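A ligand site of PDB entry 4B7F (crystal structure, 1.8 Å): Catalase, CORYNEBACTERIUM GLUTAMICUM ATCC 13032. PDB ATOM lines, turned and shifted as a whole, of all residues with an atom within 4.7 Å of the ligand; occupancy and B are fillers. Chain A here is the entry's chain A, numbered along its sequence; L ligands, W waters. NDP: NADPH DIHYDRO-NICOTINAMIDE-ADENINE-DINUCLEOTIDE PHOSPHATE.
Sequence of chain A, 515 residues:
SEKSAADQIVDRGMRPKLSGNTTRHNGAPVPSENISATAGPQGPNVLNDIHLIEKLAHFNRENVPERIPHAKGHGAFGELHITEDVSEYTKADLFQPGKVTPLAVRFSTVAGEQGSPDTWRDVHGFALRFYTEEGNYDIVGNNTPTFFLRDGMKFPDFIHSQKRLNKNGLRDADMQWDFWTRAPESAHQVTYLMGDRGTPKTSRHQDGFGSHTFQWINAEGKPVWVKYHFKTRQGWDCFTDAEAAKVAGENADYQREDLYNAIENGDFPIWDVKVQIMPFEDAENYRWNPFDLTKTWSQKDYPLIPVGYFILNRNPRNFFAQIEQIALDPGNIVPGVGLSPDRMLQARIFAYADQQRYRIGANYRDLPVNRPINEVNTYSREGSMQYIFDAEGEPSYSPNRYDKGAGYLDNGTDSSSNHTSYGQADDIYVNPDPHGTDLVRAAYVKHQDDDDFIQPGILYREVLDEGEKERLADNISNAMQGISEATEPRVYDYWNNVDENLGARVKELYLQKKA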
ATOM      1  N   PRO A 145     -21.238   8.465   3.737  1.00  0.00           N
ATOM      2  CA  PRO A 145     -21.815   8.366   2.391  1.00  0.00           C
ATOM      3  C   PRO A 145     -22.355   6.967   2.092  1.00  0.00           C
ATOM      4  O   PRO A 145     -22.991   6.769   1.052  1.00  0.00           O
ATOM      5  CB  PRO A 145     -20.602   8.643   1.477  1.00  0.00           C
ATOM      6  CG  PRO A 145     -19.425   8.128   2.280  1.00  0.00           C
ATOM      7  CD  PRO A 145     -19.762   8.484   3.711  1.00  0.00           C
ATOM      8  N   HIS A 188     -17.452  -2.028   4.111  1.00  0.00           N
ATOM      9  CA  HIS A 188     -17.257  -0.616   3.765  1.00  0.00           C
ATOM     10  C   HIS A 188     -17.587   0.330   4.947  1.00  0.00           C
ATOM     11  O   HIS A 188     -16.774   1.183   5.303  1.00  0.00           O
ATOM     12  CB  HIS A 188     -18.072  -0.224   2.516  1.00  0.00           C
ATOM     13  CG  HIS A 188     -17.626   1.060   1.878  1.00  0.00           C
ATOM     14  ND1 HIS A 188     -18.256   1.597   0.771  1.00  0.00           N
ATOM     15  CD2 HIS A 188     -16.608   1.901   2.171  1.00  0.00           C
ATOM     16  CE1 HIS A 188     -17.657   2.723   0.432  1.00  0.00           C
ATOM     17  NE2 HIS A 188     -16.651   2.921   1.258  1.00  0.00           N
ATOM     18  N   TYR A 192     -15.139   2.726   7.556  1.00  0.00           N
ATOM     19  CA  TYR A 192     -15.379   4.157   7.782  1.00  0.00           C
ATOM     20  C   TYR A 192     -15.594   4.432   9.272  1.00  0.00           C
ATOM     21  O   TYR A 192     -15.072   5.408   9.835  1.00  0.00           O
ATOM     22  CB  TYR A 192     -16.633   4.563   7.000  1.00  0.00           C
ATOM     23  CG  TYR A 192     -16.912   6.036   6.870  1.00  0.00           C
ATOM     24  CD1 TYR A 192     -17.601   6.729   7.873  1.00  0.00           C
ATOM     25  CD2 TYR A 192     -16.571   6.729   5.713  1.00  0.00           C
ATOM     26  CE1 TYR A 192     -17.894   8.076   7.752  1.00  0.00           C
ATOM     27  CE2 TYR A 192     -16.868   8.082   5.585  1.00  0.00           C
ATOM     28  CZ  TYR A 192     -17.538   8.741   6.605  1.00  0.00           C
ATOM     29  OH  TYR A 192     -17.835  10.080   6.480  1.00  0.00           O
ATOM     30  N   ASP A 196     -11.044   7.531  11.973  1.00  0.00           N
ATOM     31  CA  ASP A 196     -11.179   8.769  12.752  1.00  0.00           C
ATOM     32  C   ASP A 196     -12.623   9.256  12.811  1.00  0.00           C
ATOM     33  O   ASP A 196     -13.070   9.767  13.854  1.00  0.00           O
ATOM     34  CB  ASP A 196     -10.331   9.884  12.143  1.00  0.00           C
ATOM     35  CG  ASP A 196      -8.837   9.652  12.292  1.00  0.00           C
ATOM     36  OD1 ASP A 196      -8.440   8.685  12.960  1.00  0.00           O
ATOM     37  OD2 ASP A 196      -8.071  10.455  11.726  1.00  0.00           O
ATOM     38  N   ARG A 197     -13.336   9.129  11.705  1.00  0.00           N
ATOM     39  CA  ARG A 197     -14.671   9.710  11.573  1.00  0.00           C
ATOM     40  C   ARG A 197     -15.715   9.021  12.463  1.00  0.00           C
ATOM     41  O   ARG A 197     -16.827   9.523  12.601  1.00  0.00           O
ATOM     42  CB  ARG A 197     -15.126   9.688  10.119  1.00  0.00           C
ATOM     43  CG  ARG A 197     -14.331  10.631   9.231  1.00  0.00           C
ATOM     44  CD  ARG A 197     -14.916  10.686   7.825  1.00  0.00           C
ATOM     45  NE  ARG A 197     -14.126  11.571   6.975  1.00  0.00           N
ATOM     46  CZ  ARG A 197     -14.505  11.980   5.758  1.00  0.00           C
ATOM     47  NH1 ARG A 197     -15.672  11.601   5.240  1.00  0.00           N
ATOM     48  NH2 ARG A 197     -13.704  12.777   5.075  1.00  0.00           N
ATOM     49  N   PHE A 209     -24.554  13.309   4.650  1.00  0.00           N
ATOM     50  CA  PHE A 209     -24.804  12.708   3.338  1.00  0.00           C
ATOM     51  C   PHE A 209     -26.198  12.125   3.310  1.00  0.00           C
ATOM     52  O   PHE A 209     -26.705  11.676   4.348  1.00  0.00           O
ATOM     53  CB  PHE A 209     -23.826  11.558   3.067  1.00  0.00           C
ATOM     54  CG  PHE A 209     -22.381  11.926   3.237  1.00  0.00           C
ATOM     55  CD1 PHE A 209     -21.787  11.887   4.488  1.00  0.00           C
ATOM     56  CD2 PHE A 209     -21.612  12.295   2.127  1.00  0.00           C
ATOM     57  CE1 PHE A 209     -20.451  12.216   4.659  1.00  0.00           C
ATOM     58  CE2 PHE A 209     -20.271  12.629   2.286  1.00  0.00           C
ATOM     59  CZ  PHE A 209     -19.684  12.594   3.560  1.00  0.00           C
ATOM     60  N   HIS A 229     -24.500  15.555  -0.728  1.00  0.00           N
ATOM     61  CA  HIS A 229     -23.360  15.771   0.153  1.00  0.00           C
ATOM     62  C   HIS A 229     -23.446  17.133   0.820  1.00  0.00           C
ATOM     63  O   HIS A 229     -23.571  18.159   0.145  1.00  0.00           O
ATOM     64  CB  HIS A 229     -22.052  15.734  -0.605  1.00  0.00           C
ATOM     65  CG  HIS A 229     -21.776  14.446  -1.307  1.00  0.00           C
ATOM     66  ND1 HIS A 229     -20.814  13.634  -0.964  1.00  0.00           N
ATOM     67  CD2 HIS A 229     -22.413  13.861  -2.348  1.00  0.00           C
ATOM     68  CE1 HIS A 229     -20.845  12.597  -1.737  1.00  0.00           C
ATOM     69  NE2 HIS A 229     -21.820  12.739  -2.579  1.00  0.00           N
ATOM     70  N   LYS A 231     -21.283  19.467   2.946  1.00  0.00           N
ATOM     71  CA  LYS A 231     -19.865  19.579   3.300  1.00  0.00           C
ATOM     72  C   LYS A 231     -19.660  20.649   4.357  1.00  0.00           C
ATOM     73  O   LYS A 231     -20.017  21.820   4.157  1.00  0.00           O
ATOM     74  CB  LYS A 231     -19.041  19.865   2.048  1.00  0.00           C
ATOM     75  CG  LYS A 231     -19.379  18.948   0.887  1.00  0.00           C
ATOM     76  CD  LYS A 231     -18.965  17.516   1.167  1.00  0.00           C
ATOM     77  CE  LYS A 231     -17.450  17.412   1.364  1.00  0.00           C
ATOM     78  NZ  LYS A 231     -17.033  15.996   1.612  1.00  0.00           N
ATOM     79  N   GLN A 276     -23.896  14.789  -6.366  1.00  0.00           N
ATOM     80  CA  GLN A 276     -23.324  14.086  -7.501  1.00  0.00           C
ATOM     81  C   GLN A 276     -24.486  13.858  -8.408  1.00  0.00           C
ATOM     82  O   GLN A 276     -25.592  13.598  -7.935  1.00  0.00           O
ATOM     83  CB  GLN A 276     -22.738  12.737  -7.068  1.00  0.00           C
ATOM     84  CG  GLN A 276     -21.512  12.853  -6.170  1.00  0.00           C
ATOM     85  CD  GLN A 276     -20.979  11.501  -5.722  1.00  0.00           C
ATOM     86  OE1 GLN A 276     -21.587  10.837  -4.883  1.00  0.00           O
ATOM     87  NE2 GLN A 276     -19.838  11.092  -6.287  1.00  0.00           N
ATOM     88  N   THR A 296     -20.294   3.581  -2.755  1.00  0.00           N
ATOM     89  CA  THR A 296     -20.282   5.009  -3.093  1.00  0.00           C
ATOM     90  C   THR A 296     -19.988   5.204  -4.582  1.00  0.00           C
ATOM     91  O   THR A 296     -19.438   4.317  -5.230  1.00  0.00           O
ATOM     92  CB  THR A 296     -19.256   5.811  -2.255  1.00  0.00           C
ATOM     93  OG1 THR A 296     -17.975   5.159  -2.308  1.00  0.00           O
ATOM     94  CG2 THR A 296     -19.703   5.887  -0.808  1.00  0.00           C
ATOM     95  N   TRP A 297     -20.396   6.350  -5.121  1.00  0.00           N
ATOM     96  CA  TRP A 297     -19.967   6.758  -6.465  1.00  0.00           C
ATOM     97  C   TRP A 297     -18.630   7.483  -6.329  1.00  0.00           C
ATOM     98  O   TRP A 297     -18.504   8.396  -5.506  1.00  0.00           O
ATOM     99  CB  TRP A 297     -20.958   7.741  -7.080  1.00  0.00           C
ATOM    100  CG  TRP A 297     -22.350   7.213  -7.298  1.00  0.00           C
ATOM    101  CD1 TRP A 297     -22.795   5.920  -7.151  1.00  0.00           C
ATOM    102  CD2 TRP A 297     -23.489   7.976  -7.711  1.00  0.00           C
ATOM    103  NE1 TRP A 297     -24.138   5.849  -7.452  1.00  0.00           N
ATOM    104  CE2 TRP A 297     -24.585   7.092  -7.799  1.00  0.00           C
ATOM    105  CE3 TRP A 297     -23.687   9.340  -8.009  1.00  0.00           C
ATOM    106  CZ2 TRP A 297     -25.864   7.530  -8.175  1.00  0.00           C
ATOM    107  CZ3 TRP A 297     -24.946   9.755  -8.388  1.00  0.00           C
ATOM    108  CH2 TRP A 297     -26.021   8.865  -8.465  1.00  0.00           C
ATOM    109  N   SER A 298     -17.629   7.115  -7.115  1.00  0.00           N
ATOM    110  CA  SER A 298     -16.369   7.857  -7.065  1.00  0.00           C
ATOM    111  C   SER A 298     -16.586   9.319  -7.425  1.00  0.00           C
ATOM    112  O   SER A 298     -17.327   9.640  -8.350  1.00  0.00           O
ATOM    113  CB  SER A 298     -15.303   7.265  -7.982  1.00  0.00           C
ATOM    114  OG  SER A 298     -14.139   8.078  -7.956  1.00  0.00           O
ATOM    115  N   GLN A 299     -15.972  10.218  -6.662  1.00  0.00           N
ATOM    116  CA  GLN A 299     -16.060  11.640  -6.930  1.00  0.00           C
ATOM    117  C   GLN A 299     -15.166  12.028  -8.114  1.00  0.00           C
ATOM    118  O   GLN A 299     -15.237  13.151  -8.627  1.00  0.00           O
ATOM    119  CB  GLN A 299     -15.726  12.438  -5.666  1.00  0.00           C
ATOM    120  CG  GLN A 299     -16.751  12.208  -4.553  1.00  0.00           C
ATOM    121  CD  GLN A 299     -16.261  12.612  -3.170  1.00  0.00           C
ATOM    122  OE1 GLN A 299     -15.514  11.881  -2.512  1.00  0.00           O
ATOM    123  NE2 GLN A 299     -16.690  13.784  -2.722  1.00  0.00           N
ATOM    124  N   LYS A 300     -14.346  11.079  -8.550  1.00  0.00           N
ATOM    125  CA  LYS A 300     -13.580  11.234  -9.783  1.00  0.00           C
ATOM    126  C   LYS A 300     -14.463  10.988 -11.001  1.00  0.00           C
ATOM    127  O   LYS A 300     -14.260  11.603 -12.055  1.00  0.00           O
ATOM    128  CB  LYS A 300     -12.392  10.277  -9.793  1.00  0.00           C
ATOM    129  CG  LYS A 300     -11.210  10.879  -9.089  1.00  0.00           C
ATOM    130  CD  LYS A 300     -10.322   9.843  -8.430  1.00  0.00           C
ATOM    131  CE  LYS A 300      -9.369  10.526  -7.463  1.00  0.00           C
ATOM    132  NZ  LYS A 300      -8.157   9.707  -7.192  1.00  0.00           N
ATOM    133  N   GLN A 455     -14.225  -1.417  -2.060  1.00  0.00           N
ATOM    134  CA  GLN A 455     -14.318  -0.009  -1.675  1.00  0.00           C
ATOM    135  C   GLN A 455     -13.608   0.381  -0.365  1.00  0.00           C
ATOM    136  O   GLN A 455     -12.921   1.409  -0.324  1.00  0.00           O
ATOM    137  CB  GLN A 455     -15.758   0.502  -1.731  1.00  0.00           C
ATOM    138  CG  GLN A 455     -16.309   0.516  -3.167  1.00  0.00           C
ATOM    139  CD  GLN A 455     -17.458   1.494  -3.327  1.00  0.00           C
ATOM    140  OE1 GLN A 455     -18.151   1.808  -2.362  1.00  0.00           O
ATOM    141  NE2 GLN A 455     -17.650   1.988  -4.551  1.00  0.00           N
ATOM    142  N   ILE A 458      -9.964   0.314  -1.200  1.00  0.00           N
ATOM    143  CA  ILE A 458      -9.581   1.534  -1.888  1.00  0.00           C
ATOM    144  C   ILE A 458      -9.383   2.681  -0.891  1.00  0.00           C
ATOM    145  O   ILE A 458      -8.425   3.451  -1.004  1.00  0.00           O
ATOM    146  CB  ILE A 458     -10.617   1.920  -2.960  1.00  0.00           C
ATOM    147  CG1 ILE A 458     -10.550   0.955  -4.148  1.00  0.00           C
ATOM    148  CG2 ILE A 458     -10.390   3.361  -3.435  1.00  0.00           C
ATOM    149  CD1 ILE A 458     -11.711   1.111  -5.117  1.00  0.00           C
ATOM    150  N   LEU A 459     -10.306   2.788   0.069  1.00  0.00           N
ATOM    151  CA  LEU A 459     -10.202   3.815   1.102  1.00  0.00           C
ATOM    152  C   LEU A 459      -8.872   3.672   1.843  1.00  0.00           C
ATOM    153  O   LEU A 459      -8.136   4.642   2.026  1.00  0.00           O
ATOM    154  CB  LEU A 459     -11.372   3.678   2.091  1.00  0.00           C
ATOM    155  CG  LEU A 459     -11.379   4.533   3.364  1.00  0.00           C
ATOM    156  CD1 LEU A 459     -11.376   6.013   3.036  1.00  0.00           C
ATOM    157  CD2 LEU A 459     -12.568   4.171   4.245  1.00  0.00           C
ATOM    158  N   VAL A 463      -6.681   6.419  -0.131  1.00  0.00           N
ATOM    159  CA  VAL A 463      -7.237   7.638   0.440  1.00  0.00           C
ATOM    160  C   VAL A 463      -6.628   7.989   1.790  1.00  0.00           C
ATOM    161  O   VAL A 463      -6.214   9.129   2.015  1.00  0.00           O
ATOM    162  CB  VAL A 463      -8.764   7.536   0.599  1.00  0.00           C
ATOM    163  CG1 VAL A 463      -9.322   8.795   1.239  1.00  0.00           C
ATOM    164  CG2 VAL A 463      -9.437   7.294  -0.759  1.00  0.00           C
ATOM    165  N   LEU A 464      -6.573   7.014   2.678  1.00  0.00           N
ATOM    166  CA  LEU A 464      -6.132   7.273   4.047  1.00  0.00           C
ATOM    167  C   LEU A 464      -4.643   7.583   4.090  1.00  0.00           C
ATOM    168  O   LEU A 464      -3.859   6.966   3.356  1.00  0.00           O
ATOM    169  CB  LEU A 464      -6.423   6.054   4.935  1.00  0.00           C
ATOM    170  CG  LEU A 464      -7.891   5.664   5.150  1.00  0.00           C
ATOM    171  CD1 LEU A 464      -7.974   4.547   6.185  1.00  0.00           C
ATOM    172  CD2 LEU A 464      -8.690   6.885   5.587  1.00  0.00           C
ATOM    173  N   GLU A 468      -3.859   7.836   9.635  1.00  0.00           N
ATOM    174  CA  GLU A 468      -5.237   7.346   9.609  1.00  0.00           C
ATOM    175  C   GLU A 468      -5.253   5.825   9.518  1.00  0.00           C
ATOM    176  O   GLU A 468      -6.075   5.166  10.163  1.00  0.00           O
ATOM    177  CB  GLU A 468      -6.010   7.942   8.436  1.00  0.00           C
ATOM    178  CG  GLU A 468      -6.288   9.423   8.568  1.00  0.00           C
ATOM    179  CD  GLU A 468      -6.911   9.999   7.313  1.00  0.00           C
ATOM    180  OE1 GLU A 468      -6.368   9.770   6.219  1.00  0.00           O
ATOM    181  OE2 GLU A 468      -7.955  10.687   7.417  1.00  0.00           O
HETATM  182  PA  NDP L   1     -11.846  10.691  -3.634  1.00  0.00           P
HETATM  183  O1A NDP L   1     -10.379  10.892  -3.513  1.00  0.00           O
HETATM  184  O2A NDP L   1     -12.429  11.515  -4.726  1.00  0.00           O
HETATM  185  O5B NDP L   1     -12.452  11.059  -2.190  1.00  0.00           O
HETATM  186  C5B NDP L   1     -12.159  10.225  -1.092  1.00  0.00           C
HETATM  187  C4B NDP L   1     -13.079  10.667   0.029  1.00  0.00           C
HETATM  188  O4B NDP L   1     -12.726  10.046   1.259  1.00  0.00           O
HETATM  189  C3B NDP L   1     -13.001  12.186   0.217  1.00  0.00           C
HETATM  190  O3B NDP L   1     -14.298  12.737   0.304  1.00  0.00           O
HETATM  191  C2B NDP L   1     -12.301  12.322   1.551  1.00  0.00           C
HETATM  192  O2B NDP L   1     -12.619  13.504   2.254  1.00  0.00           O
HETATM  193  C1B NDP L   1     -12.727  11.036   2.264  1.00  0.00           C
HETATM  194  N9A NDP L   1     -11.891  10.739   3.438  1.00  0.00           N
HETATM  195  C8A NDP L   1     -10.650  11.245   3.744  1.00  0.00           C
HETATM  196  N7A NDP L   1     -10.249  10.722   4.931  1.00  0.00           N
HETATM  197  C5A NDP L   1     -11.223   9.887   5.385  1.00  0.00           C
HETATM  198  C6A NDP L   1     -11.343   9.091   6.534  1.00  0.00           C
HETATM  199  N6A NDP L   1     -10.539   9.304   7.574  1.00  0.00           N
HETATM  200  N1A NDP L   1     -12.482   8.331   6.709  1.00  0.00           N
HETATM  201  C2A NDP L   1     -13.488   8.362   5.752  1.00  0.00           C
HETATM  202  N3A NDP L   1     -13.367   9.146   4.622  1.00  0.00           N
HETATM  203  C4A NDP L   1     -12.253   9.894   4.450  1.00  0.00           C
HETATM  204  O3  NDP L   1     -12.130   9.112  -3.795  1.00  0.00           O
HETATM  205  PN  NDP L   1     -13.547   8.437  -4.210  1.00  0.00           P
HETATM  206  O1N NDP L   1     -14.639   9.451  -4.221  1.00  0.00           O
HETATM  207  O2N NDP L   1     -13.340   7.561  -5.385  1.00  0.00           O
HETATM  208  O5D NDP L   1     -13.765   7.413  -2.989  1.00  0.00           O
HETATM  209  C5D NDP L   1     -12.649   6.772  -2.401  1.00  0.00           C
HETATM  210  C4D NDP L   1     -13.054   6.231  -1.031  1.00  0.00           C
HETATM  211  O4D NDP L   1     -13.352   7.299  -0.146  1.00  0.00           O
HETATM  212  C3D NDP L   1     -14.316   5.388  -1.129  1.00  0.00           C
HETATM  213  O3D NDP L   1     -14.037   4.010  -1.330  1.00  0.00           O
HETATM  214  C2D NDP L   1     -15.023   5.653   0.191  1.00  0.00           C
HETATM  215  O2D NDP L   1     -14.659   4.666   1.116  1.00  0.00           O
HETATM  216  C1D NDP L   1     -14.452   6.970   0.695  1.00  0.00           C
HETATM  217  N1N NDP L   1     -15.468   8.048   0.652  1.00  0.00           N
HETATM  218  C2N NDP L   1     -16.206   8.226  -0.485  1.00  0.00           C
HETATM  219  C3N NDP L   1     -17.073   9.293  -0.646  1.00  0.00           C
HETATM  220  C7N NDP L   1     -17.842   9.396  -1.938  1.00  0.00           C
HETATM  221  O7N NDP L   1     -19.165   9.875  -1.902  1.00  0.00           O
HETATM  222  N7N NDP L   1     -17.276   9.028  -3.087  1.00  0.00           N
HETATM  223  C4N NDP L   1     -17.273  10.333   0.438  1.00  0.00           C
HETATM  224  C5N NDP L   1     -16.422  10.047   1.644  1.00  0.00           C
HETATM  225  C6N NDP L   1     -15.570   8.934   1.696  1.00  0.00           C
HETATM  226  P2B NDP L   1     -11.709  14.829   2.059  1.00  0.00           P
HETATM  227  O1X NDP L   1     -10.263  14.550   2.435  1.00  0.00           O
HETATM  228  O2X NDP L   1     -11.787  15.329   0.635  1.00  0.00           O
HETATM  229  O3X NDP L   1     -12.254  15.881   3.008  1.00  0.00           O
HETATM  230  O   HOH W   1     -21.122   8.749  -3.263  1.00  0.00           O
HETATM  231  O   HOH W   2     -13.034   7.133   9.149  1.00  0.00           O
HETATM  232  O   HOH W   3     -14.499   3.803  -4.218  1.00  0.00           O
HETATM  233  O   HOH W   4      -7.963  11.721   5.246  1.00  0.00           O
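OG of Ser 298 lies within hydrogen-bond range of O2N of the ligand (2.7 Å). N7N of the ligand lies within hydrogen-bond range of O of Trp 297 (2.8 Å). An oxygen (O1N) of the ligand sits at hydrogen-bond distance from the backbone NH of Gln 299. OE2 of Glu 468 lies within hydrogen-bond range of N6A of the ligand (2.9 Å). The guanidinium group (NH2) of Arg 197 lies within hydrogen-bond range of an oxygen (O2B) of the ligand (3.1 Å). An oxygen (O3D) of the ligand sits at hydrogen-bond distance from the backbone carbonyl oxygen of Gln 455, 3.0 Å away. An oxygen (O2D) of the ligand sits at hydrogen-bond distance from a ring nitrogen (NE2) of His 188 (2.7 Å). The side-chain amide oxygen of Gln 299 lies close to an oxygen (O1N) of the ligand.
The backbone NH of Leu 464 is in hydrogen-bond range of the backbone carbonyl oxygen of Leu 459, at 2.9 Å. The side-chain hydroxyl of Tyr 192 is in hydrogen-bond range of the guanidinium group of Arg 197, at 2.9 Å. The side-chain hydroxyl of Ser 298 lies close to the backbone NH of Lys 300, at 3.1 Å. A ring nitrogen (NE2) of His 229 lies within hydrogen-bond range of the side-chain amide oxygen of Gln 276 (3.0 Å). A ring nitrogen (ND1) of His 188 lies close to the side-chain amide oxygen of Gln 455 (3.1 Å). The side-chain amide oxygen (OE1) of Gln 455 is in hydrogen-bond range of the backbone NH (N) of Thr 296, 2.8 Å away. The side-chain amide nitrogen of Gln 276 lies within hydrogen-bond range of the backbone carbonyl oxygen of Trp 297 (3.1 Å).
CG of Pro 145 touches C4N of the ligand, 3.6 Å away. Tyr 192 touches the ligand. His 229 touches the ligand. Gln 276 touches the ligand. Thr 296 touches the ligand. CB of Leu 459 touches O2D of the ligand, at 3.6 Å. CG1 of Val 463 touches O4B of the ligand, at 3.6 Å. Leu 464 touches the ligand. Within 4 Å of the ligand: Pro 145, His 188, Tyr 192, Arg 197, His 229, Gln 276, Thr 296, Trp 297, Ser 298, Gln 299, Gln 455, Leu 459, Val 463, Leu 464 and Glu 468. The nearest printed residue that does not touch the ligand is Lys 300 (4.1 Å).
Water W4 bridges OE2 of Glu 468 and N7A of the ligand. Water W1 lies within hydrogen-bond range of O7N of the ligand (2.6 Å), OE1 of Gln 276 (2.7 Å) and N of Trp 297 (3.1 Å). Water W2 lies within hydrogen-bond range of the backbone carbonyl oxygen (O) of Tyr 192 (2.8 Å), a nitrogen (N1A) of the ligand (2.8 Å), the backbone NH (N) of Arg 197 (3.3 Å) and the backbone NH (N) of Asp 196 (3.5 Å).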
